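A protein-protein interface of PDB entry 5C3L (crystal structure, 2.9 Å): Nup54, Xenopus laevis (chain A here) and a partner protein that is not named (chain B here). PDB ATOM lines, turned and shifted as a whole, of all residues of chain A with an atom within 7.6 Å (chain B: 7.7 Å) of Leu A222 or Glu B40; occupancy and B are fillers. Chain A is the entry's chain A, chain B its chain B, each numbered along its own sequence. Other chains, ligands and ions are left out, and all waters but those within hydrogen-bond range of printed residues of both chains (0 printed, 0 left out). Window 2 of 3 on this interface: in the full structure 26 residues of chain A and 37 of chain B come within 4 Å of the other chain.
Among the printed residues, pairs that only touch across the chains: Phe A218 with Gln B34 (3.6 Å), Phe A218 with Val B37 (3.3 Å), Leu A222 with Glu B40 (3.4 Å), Leu A222 with Ile B41 (3.7 Å) and Leu A225 with Met B44 (3.6 Å).
Printed residues of chain B within 4 Å of Phe A218: Gln B34 and Val B37.
Of the printed residues of chain B, Leu A222 touches Glu B40 and Ile B41.
Of the printed residues of chain B, Leu A225 touches Met B44 (3.6 Å).
Of the printed residues of chain A, Gln B34 touches Phe A218 (3.6 Å).
Glu B40 touches one residue of chain A.
Printed residues of chain A within 4 Å of Ile B41: Leu A222.
Arg B43 touches none of the printed residues of chain A.
The nearest residue of chain B that does not touch Leu A222 is Met B44 (4.4 Å).
The nearest residue of chain A that does not touch Glu B40 is Glu A226 (5.5 Å).
Of the 12 printed residues of chain A, 3 touch a printed residue of chain B.
Printed residues of chain A that touch a printed residue of chain B: Phe A218, Leu A222 and Leu A225.
Hydrophobic or aromatic side chains of chain A that line the printed part of chain B: Phe A218, Leu A222 and Leu A225.
Printed residues of chain B that touch a printed residue of chain A: Gln B34, Val B37, Glu B40, Ile B41 and Met B44.
Along chain B the printed residues that touch a printed residue of chain A span positions 34 to 44.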
ATOM      1  N   GLY A 217      32.319 -18.029   9.402  1.00  0.00           N
ATOM      2  CA  GLY A 217      31.864 -19.375   9.109  1.00  0.00           C
ATOM      3  C   GLY A 217      30.721 -19.852   9.986  1.00  0.00           C
ATOM      4  O   GLY A 217      30.605 -19.457  11.151  1.00  0.00           O
ATOM      5  N   PHE A 218      29.880 -20.718   9.420  1.00  0.00           N
ATOM      6  CA  PHE A 218      28.792 -21.357  10.149  1.00  0.00           C
ATOM      7  C   PHE A 218      29.284 -22.125  11.391  1.00  0.00           C
ATOM      8  O   PHE A 218      28.488 -22.457  12.276  1.00  0.00           O
ATOM      9  CB  PHE A 218      28.025 -22.314   9.228  1.00  0.00           C
ATOM     10  CG  PHE A 218      27.181 -21.623   8.185  1.00  0.00           C
ATOM     11  CD1 PHE A 218      26.103 -20.836   8.550  1.00  0.00           C
ATOM     12  CD2 PHE A 218      27.453 -21.776   6.835  1.00  0.00           C
ATOM     13  CE1 PHE A 218      25.326 -20.206   7.589  1.00  0.00           C
ATOM     14  CE2 PHE A 218      26.675 -21.143   5.871  1.00  0.00           C
ATOM     15  CZ  PHE A 218      25.616 -20.361   6.251  1.00  0.00           C
ATOM     16  N   LYS A 219      30.585 -22.400  11.460  1.00  0.00           N
ATOM     17  CA  LYS A 219      31.144 -23.156  12.582  1.00  0.00           C
ATOM     18  C   LYS A 219      31.227 -22.308  13.850  1.00  0.00           C
ATOM     19  O   LYS A 219      30.748 -22.727  14.903  1.00  0.00           O
ATOM     20  CB  LYS A 219      32.527 -23.709  12.227  1.00  0.00           C
ATOM     21  CG  LYS A 219      32.951 -24.931  13.056  1.00  0.00           C
ATOM     22  CD  LYS A 219      33.176 -24.580  14.533  1.00  0.00           C
ATOM     23  CE  LYS A 219      33.910 -25.679  15.285  1.00  0.00           C
ATOM     24  NZ  LYS A 219      34.265 -25.273  16.680  1.00  0.00           N
ATOM     25  N   GLU A 220      31.837 -21.129  13.770  1.00  0.00           N
ATOM     26  CA  GLU A 220      31.865 -20.241  14.931  1.00  0.00           C
ATOM     27  C   GLU A 220      30.430 -19.887  15.330  1.00  0.00           C
ATOM     28  O   GLU A 220      30.140 -19.657  16.502  1.00  0.00           O
ATOM     29  CB  GLU A 220      32.671 -18.969  14.649  1.00  0.00           C
ATOM     30  N   LEU A 221      29.535 -19.875  14.349  1.00  0.00           N
ATOM     31  CA  LEU A 221      28.137 -19.537  14.583  1.00  0.00           C
ATOM     32  C   LEU A 221      27.467 -20.600  15.448  1.00  0.00           C
ATOM     33  O   LEU A 221      26.596 -20.303  16.269  1.00  0.00           O
ATOM     34  CB  LEU A 221      27.401 -19.392  13.251  1.00  0.00           C
ATOM     35  CG  LEU A 221      26.706 -18.053  12.987  1.00  0.00           C
ATOM     36  CD1 LEU A 221      27.677 -16.871  13.037  1.00  0.00           C
ATOM     37  CD2 LEU A 221      25.972 -18.107  11.642  1.00  0.00           C
ATOM     38  N   LEU A 222      27.884 -21.845  15.256  1.00  0.00           N
ATOM     39  CA  LEU A 222      27.341 -22.964  16.006  1.00  0.00           C
ATOM     40  C   LEU A 222      28.067 -23.063  17.335  1.00  0.00           C
ATOM     41  O   LEU A 222      27.487 -23.436  18.350  1.00  0.00           O
ATOM     42  CB  LEU A 222      27.490 -24.263  15.217  1.00  0.00           C
ATOM     43  CG  LEU A 222      26.762 -25.479  15.794  1.00  0.00           C
ATOM     44  CD1 LEU A 222      25.269 -25.436  15.452  1.00  0.00           C
ATOM     45  CD2 LEU A 222      27.405 -26.774  15.309  1.00  0.00           C
ATOM     46  N   ARG A 223      29.350 -22.722  17.321  1.00  0.00           N
ATOM     47  CA  ARG A 223      30.158 -22.772  18.533  1.00  0.00           C
ATOM     48  C   ARG A 223      29.543 -21.819  19.549  1.00  0.00           C
ATOM     49  O   ARG A 223      29.379 -22.163  20.715  1.00  0.00           O
ATOM     50  CB  ARG A 223      31.622 -22.407  18.244  1.00  0.00           C
ATOM     51  CG  ARG A 223      32.597 -22.795  19.356  1.00  0.00           C
ATOM     52  CD  ARG A 223      32.864 -21.625  20.299  1.00  0.00           C
ATOM     53  NE  ARG A 223      33.520 -20.518  19.609  1.00  0.00           N
ATOM     54  CZ  ARG A 223      33.557 -19.263  20.051  1.00  0.00           C
ATOM     55  NH1 ARG A 223      32.971 -18.926  21.192  1.00  0.00           N
ATOM     56  NH2 ARG A 223      34.180 -18.336  19.338  1.00  0.00           N
ATOM     57  N   ARG A 224      29.181 -20.628  19.081  1.00  0.00           N
ATOM     58  CA  ARG A 224      28.532 -19.627  19.920  1.00  0.00           C
ATOM     59  C   ARG A 224      27.159 -20.096  20.393  1.00  0.00           C
ATOM     60  O   ARG A 224      26.759 -19.848  21.529  1.00  0.00           O
ATOM     61  CB  ARG A 224      28.399 -18.311  19.158  1.00  0.00           C
ATOM     62  CG  ARG A 224      29.717 -17.577  18.974  1.00  0.00           C
ATOM     63  CD  ARG A 224      29.530 -16.072  19.041  1.00  0.00           C
ATOM     64  NE  ARG A 224      30.810 -15.377  19.078  1.00  0.00           N
ATOM     65  CZ  ARG A 224      31.028 -14.212  19.679  1.00  0.00           C
ATOM     66  NH1 ARG A 224      30.056 -13.581  20.321  1.00  0.00           N
ATOM     67  NH2 ARG A 224      32.238 -13.677  19.644  1.00  0.00           N
ATOM     68  N   LEU A 225      26.440 -20.775  19.513  1.00  0.00           N
ATOM     69  CA  LEU A 225      25.111 -21.264  19.834  1.00  0.00           C
ATOM     70  C   LEU A 225      25.200 -22.277  20.969  1.00  0.00           C
ATOM     71  O   LEU A 225      24.369 -22.291  21.872  1.00  0.00           O
ATOM     72  CB  LEU A 225      24.466 -21.892  18.591  1.00  0.00           C
ATOM     73  CG  LEU A 225      23.082 -21.389  18.181  1.00  0.00           C
ATOM     74  CD1 LEU A 225      22.087 -21.629  19.308  1.00  0.00           C
ATOM     75  CD2 LEU A 225      23.106 -19.913  17.780  1.00  0.00           C
ATOM     76  N   GLU A 226      26.228 -23.116  20.924  1.00  0.00           N
ATOM     77  CA  GLU A 226      26.373 -24.194  21.895  1.00  0.00           C
ATOM     78  C   GLU A 226      26.873 -23.655  23.227  1.00  0.00           C
ATOM     79  O   GLU A 226      26.568 -24.209  24.286  1.00  0.00           O
ATOM     80  CB  GLU A 226      27.323 -25.268  21.365  1.00  0.00           C
ATOM     81  CG  GLU A 226      26.680 -26.199  20.353  1.00  0.00           C
ATOM     82  CD  GLU A 226      27.668 -27.171  19.740  1.00  0.00           C
ATOM     83  OE1 GLU A 226      28.764 -26.726  19.323  1.00  0.00           O
ATOM     84  OE2 GLU A 226      27.353 -28.380  19.681  1.00  0.00           O
ATOM     85  N   VAL A 227      27.631 -22.564  23.173  1.00  0.00           N
ATOM     86  CA  VAL A 227      28.070 -21.890  24.388  1.00  0.00           C
ATOM     87  C   VAL A 227      26.836 -21.329  25.102  1.00  0.00           C
ATOM     88  O   VAL A 227      26.697 -21.474  26.316  1.00  0.00           O
ATOM     89  CB  VAL A 227      29.097 -20.764  24.084  1.00  0.00           C
ATOM     90  CG1 VAL A 227      29.324 -19.884  25.300  1.00  0.00           C
ATOM     91  CG2 VAL A 227      30.416 -21.359  23.648  1.00  0.00           C
ATOM     92  N   GLN A 228      25.936 -20.715  24.337  1.00  0.00           N
ATOM     93  CA  GLN A 228      24.695 -20.177  24.885  1.00  0.00           C
ATOM     94  C   GLN A 228      23.926 -21.230  25.644  1.00  0.00           C
ATOM     95  O   GLN A 228      23.380 -20.964  26.705  1.00  0.00           O
ATOM     96  CB  GLN A 228      23.802 -19.622  23.780  1.00  0.00           C
ATOM     97  CG  GLN A 228      24.292 -18.341  23.136  1.00  0.00           C
ATOM     98  CD  GLN A 228      23.337 -17.824  22.080  1.00  0.00           C
ATOM     99  OE1 GLN A 228      22.275 -18.412  21.829  1.00  0.00           O
ATOM    100  NE2 GLN A 228      23.704 -16.713  21.460  1.00  0.00           N
ATOM    101  N   GLU B  33      29.083 -29.951   4.708  1.00  0.00           N
ATOM    102  CA  GLU B  33      29.497 -29.572   6.057  1.00  0.00           C
ATOM    103  C   GLU B  33      28.861 -28.240   6.438  1.00  0.00           C
ATOM    104  O   GLU B  33      28.265 -28.109   7.503  1.00  0.00           O
ATOM    105  CB  GLU B  33      31.024 -29.481   6.150  1.00  0.00           C
ATOM    106  CG  GLU B  33      31.758 -30.823   6.044  1.00  0.00           C
ATOM    107  CD  GLU B  33      32.031 -31.472   7.396  1.00  0.00           C
ATOM    108  OE1 GLU B  33      32.928 -32.341   7.463  1.00  0.00           O
ATOM    109  OE2 GLU B  33      31.355 -31.119   8.386  1.00  0.00           O
ATOM    110  N   GLN B  34      28.961 -27.267   5.536  1.00  0.00           N
ATOM    111  CA  GLN B  34      28.392 -25.941   5.759  1.00  0.00           C
ATOM    112  C   GLN B  34      26.872 -25.969   5.647  1.00  0.00           C
ATOM    113  O   GLN B  34      26.187 -25.068   6.136  1.00  0.00           O
ATOM    114  CB  GLN B  34      28.977 -24.929   4.763  1.00  0.00           C
ATOM    115  CG  GLN B  34      30.140 -24.103   5.316  1.00  0.00           C
ATOM    116  CD  GLN B  34      31.225 -24.969   5.913  1.00  0.00           C
ATOM    117  OE1 GLN B  34      31.341 -26.146   5.583  1.00  0.00           O
ATOM    118  NE2 GLN B  34      32.020 -24.397   6.807  1.00  0.00           N
ATOM    119  N   LYS B  35      26.348 -27.006   5.007  1.00  0.00           N
ATOM    120  CA  LYS B  35      24.909 -27.140   4.839  1.00  0.00           C
ATOM    121  C   LYS B  35      24.301 -27.872   6.028  1.00  0.00           C
ATOM    122  O   LYS B  35      23.209 -27.533   6.477  1.00  0.00           O
ATOM    123  CB  LYS B  35      24.580 -27.881   3.540  1.00  0.00           C
ATOM    124  CG  LYS B  35      23.174 -27.631   3.024  1.00  0.00           C
ATOM    125  CD  LYS B  35      22.999 -26.182   2.603  1.00  0.00           C
ATOM    126  CE  LYS B  35      21.665 -25.956   1.925  1.00  0.00           C
ATOM    127  NZ  LYS B  35      20.526 -26.091   2.873  1.00  0.00           N
ATOM    128  N   GLN B  36      25.014 -28.868   6.542  1.00  0.00           N
ATOM    129  CA  GLN B  36      24.487 -29.688   7.625  1.00  0.00           C
ATOM    130  C   GLN B  36      24.638 -28.984   8.980  1.00  0.00           C
ATOM    131  O   GLN B  36      23.932 -29.312   9.931  1.00  0.00           O
ATOM    132  CB  GLN B  36      25.164 -31.067   7.634  1.00  0.00           C
ATOM    133  CG  GLN B  36      26.671 -31.062   7.838  1.00  0.00           C
ATOM    134  CD  GLN B  36      27.314 -32.387   7.446  1.00  0.00           C
ATOM    135  OE1 GLN B  36      26.646 -33.293   6.948  1.00  0.00           O
ATOM    136  NE2 GLN B  36      28.618 -32.503   7.674  1.00  0.00           N
ATOM    137  N   VAL B  37      25.538 -28.008   9.062  1.00  0.00           N
ATOM    138  CA  VAL B  37      25.594 -27.141  10.236  1.00  0.00           C
ATOM    139  C   VAL B  37      24.481 -26.111  10.134  1.00  0.00           C
ATOM    140  O   VAL B  37      23.802 -25.831  11.115  1.00  0.00           O
ATOM    141  CB  VAL B  37      26.960 -26.414  10.396  1.00  0.00           C
ATOM    142  CG1 VAL B  37      28.070 -27.415  10.706  1.00  0.00           C
ATOM    143  CG2 VAL B  37      27.287 -25.564   9.170  1.00  0.00           C
ATOM    144  N   GLN B  38      24.285 -25.555   8.941  1.00  0.00           N
ATOM    145  CA  GLN B  38      23.244 -24.557   8.740  1.00  0.00           C
ATOM    146  C   GLN B  38      21.906 -25.123   9.169  1.00  0.00           C
ATOM    147  O   GLN B  38      21.026 -24.390   9.614  1.00  0.00           O
ATOM    148  CB  GLN B  38      23.173 -24.110   7.281  1.00  0.00           C
ATOM    149  CG  GLN B  38      22.113 -23.045   7.026  1.00  0.00           C
ATOM    150  CD  GLN B  38      20.941 -23.556   6.211  1.00  0.00           C
ATOM    151  OE1 GLN B  38      20.746 -23.142   5.071  1.00  0.00           O
ATOM    152  NE2 GLN B  38      20.143 -24.445   6.794  1.00  0.00           N
ATOM    153  N   GLU B  39      21.755 -26.434   9.020  1.00  0.00           N
ATOM    154  CA  GLU B  39      20.545 -27.106   9.458  1.00  0.00           C
ATOM    155  C   GLU B  39      20.541 -27.225  10.977  1.00  0.00           C
ATOM    156  O   GLU B  39      19.490 -27.116  11.605  1.00  0.00           O
ATOM    157  CB  GLU B  39      20.421 -28.484   8.802  1.00  0.00           C
ATOM    158  CG  GLU B  39      20.144 -28.432   7.300  1.00  0.00           C
ATOM    159  CD  GLU B  39      18.814 -27.775   6.972  1.00  0.00           C
ATOM    160  OE1 GLU B  39      17.959 -27.672   7.878  1.00  0.00           O
ATOM    161  OE2 GLU B  39      18.620 -27.357   5.810  1.00  0.00           O
ATOM    162  N   GLU B  40      21.718 -27.440  11.562  1.00  0.00           N
ATOM    163  CA  GLU B  40      21.857 -27.497  13.016  1.00  0.00           C
ATOM    164  C   GLU B  40      21.498 -26.154  13.657  1.00  0.00           C
ATOM    165  O   GLU B  40      20.816 -26.120  14.681  1.00  0.00           O
ATOM    166  CB  GLU B  40      23.276 -27.907  13.413  1.00  0.00           C
ATOM    167  CG  GLU B  40      23.572 -29.378  13.216  1.00  0.00           C
ATOM    168  CD  GLU B  40      25.011 -29.732  13.540  1.00  0.00           C
ATOM    169  OE1 GLU B  40      25.717 -30.247  12.645  1.00  0.00           O
ATOM    170  OE2 GLU B  40      25.438 -29.491  14.690  1.00  0.00           O
ATOM    171  N   ILE B  41      21.944 -25.053  13.060  1.00  0.00           N
ATOM    172  CA  ILE B  41      21.534 -23.737  13.533  1.00  0.00           C
ATOM    173  C   ILE B  41      20.022 -23.598  13.437  1.00  0.00           C
ATOM    174  O   ILE B  41      19.377 -23.061  14.340  1.00  0.00           O
ATOM    175  CB  ILE B  41      22.163 -22.579  12.730  1.00  0.00           C
ATOM    176  CG1 ILE B  41      23.637 -22.373  13.099  1.00  0.00           C
ATOM    177  CG2 ILE B  41      21.395 -21.287  13.018  1.00  0.00           C
ATOM    178  CD1 ILE B  41      24.583 -23.381  12.511  1.00  0.00           C
ATOM    179  N   SER B  42      19.473 -24.077  12.324  1.00  0.00           N
ATOM    180  CA  SER B  42      18.044 -23.967  12.042  1.00  0.00           C
ATOM    181  C   SER B  42      17.202 -24.744  13.057  1.00  0.00           C
ATOM    182  O   SER B  42      16.010 -24.486  13.215  1.00  0.00           O
ATOM    183  CB  SER B  42      17.744 -24.470  10.628  1.00  0.00           C
ATOM    184  OG  SER B  42      18.613 -23.882   9.678  1.00  0.00           O
ATOM    185  N   ARG B  43      17.832 -25.687  13.746  1.00  0.00           N
ATOM    186  CA  ARG B  43      17.142 -26.537  14.707  1.00  0.00           C
ATOM    187  C   ARG B  43      17.061 -25.894  16.089  1.00  0.00           C
ATOM    188  O   ARG B  43      16.082 -26.076  16.812  1.00  0.00           O
ATOM    189  CB  ARG B  43      17.849 -27.890  14.797  1.00  0.00           C
ATOM    190  CG  ARG B  43      17.593 -28.789  13.601  1.00  0.00           C
ATOM    191  CD  ARG B  43      18.679 -29.840  13.466  1.00  0.00           C
ATOM    192  NE  ARG B  43      18.389 -30.814  12.417  1.00  0.00           N
ATOM    193  CZ  ARG B  43      19.140 -31.882  12.167  1.00  0.00           C
ATOM    194  NH1 ARG B  43      20.229 -32.112  12.892  1.00  0.00           N
ATOM    195  NH2 ARG B  43      18.804 -32.719  11.197  1.00  0.00           N
ATOM    196  N   MET B  44      18.085 -25.127  16.446  1.00  0.00           N
ATOM    197  CA  MET B  44      18.186 -24.556  17.785  1.00  0.00           C
ATOM    198  C   MET B  44      17.154 -23.451  17.978  1.00  0.00           C
ATOM    199  O   MET B  44      16.802 -22.745  17.028  1.00  0.00           O
ATOM    200  CB  MET B  44      19.600 -24.017  18.034  1.00  0.00           C
ATOM    201  CG  MET B  44      20.691 -24.896  17.447  1.00  0.00           C
ATOM    202  SD  MET B  44      22.136 -25.090  18.501  1.00  0.00           S
ATOM    203  CE  MET B  44      21.570 -26.347  19.638  1.00  0.00           C
ATOM    204  N   SER B  45      16.664 -23.318  19.210  1.00  0.00           N
ATOM    205  CA  SER B  45      15.736 -22.250  19.564  1.00  0.00           C
ATOM    206  C   SER B  45      16.223 -21.513  20.797  1.00  0.00           C
ATOM    207  O   SER B  45      17.316 -21.771  21.299  1.00  0.00           O
ATOM    208  CB  SER B  45      14.328 -22.803  19.792  1.00  0.00           C
ATOM    209  OG  SER B  45      13.678 -22.994  18.547  1.00  0.00           O
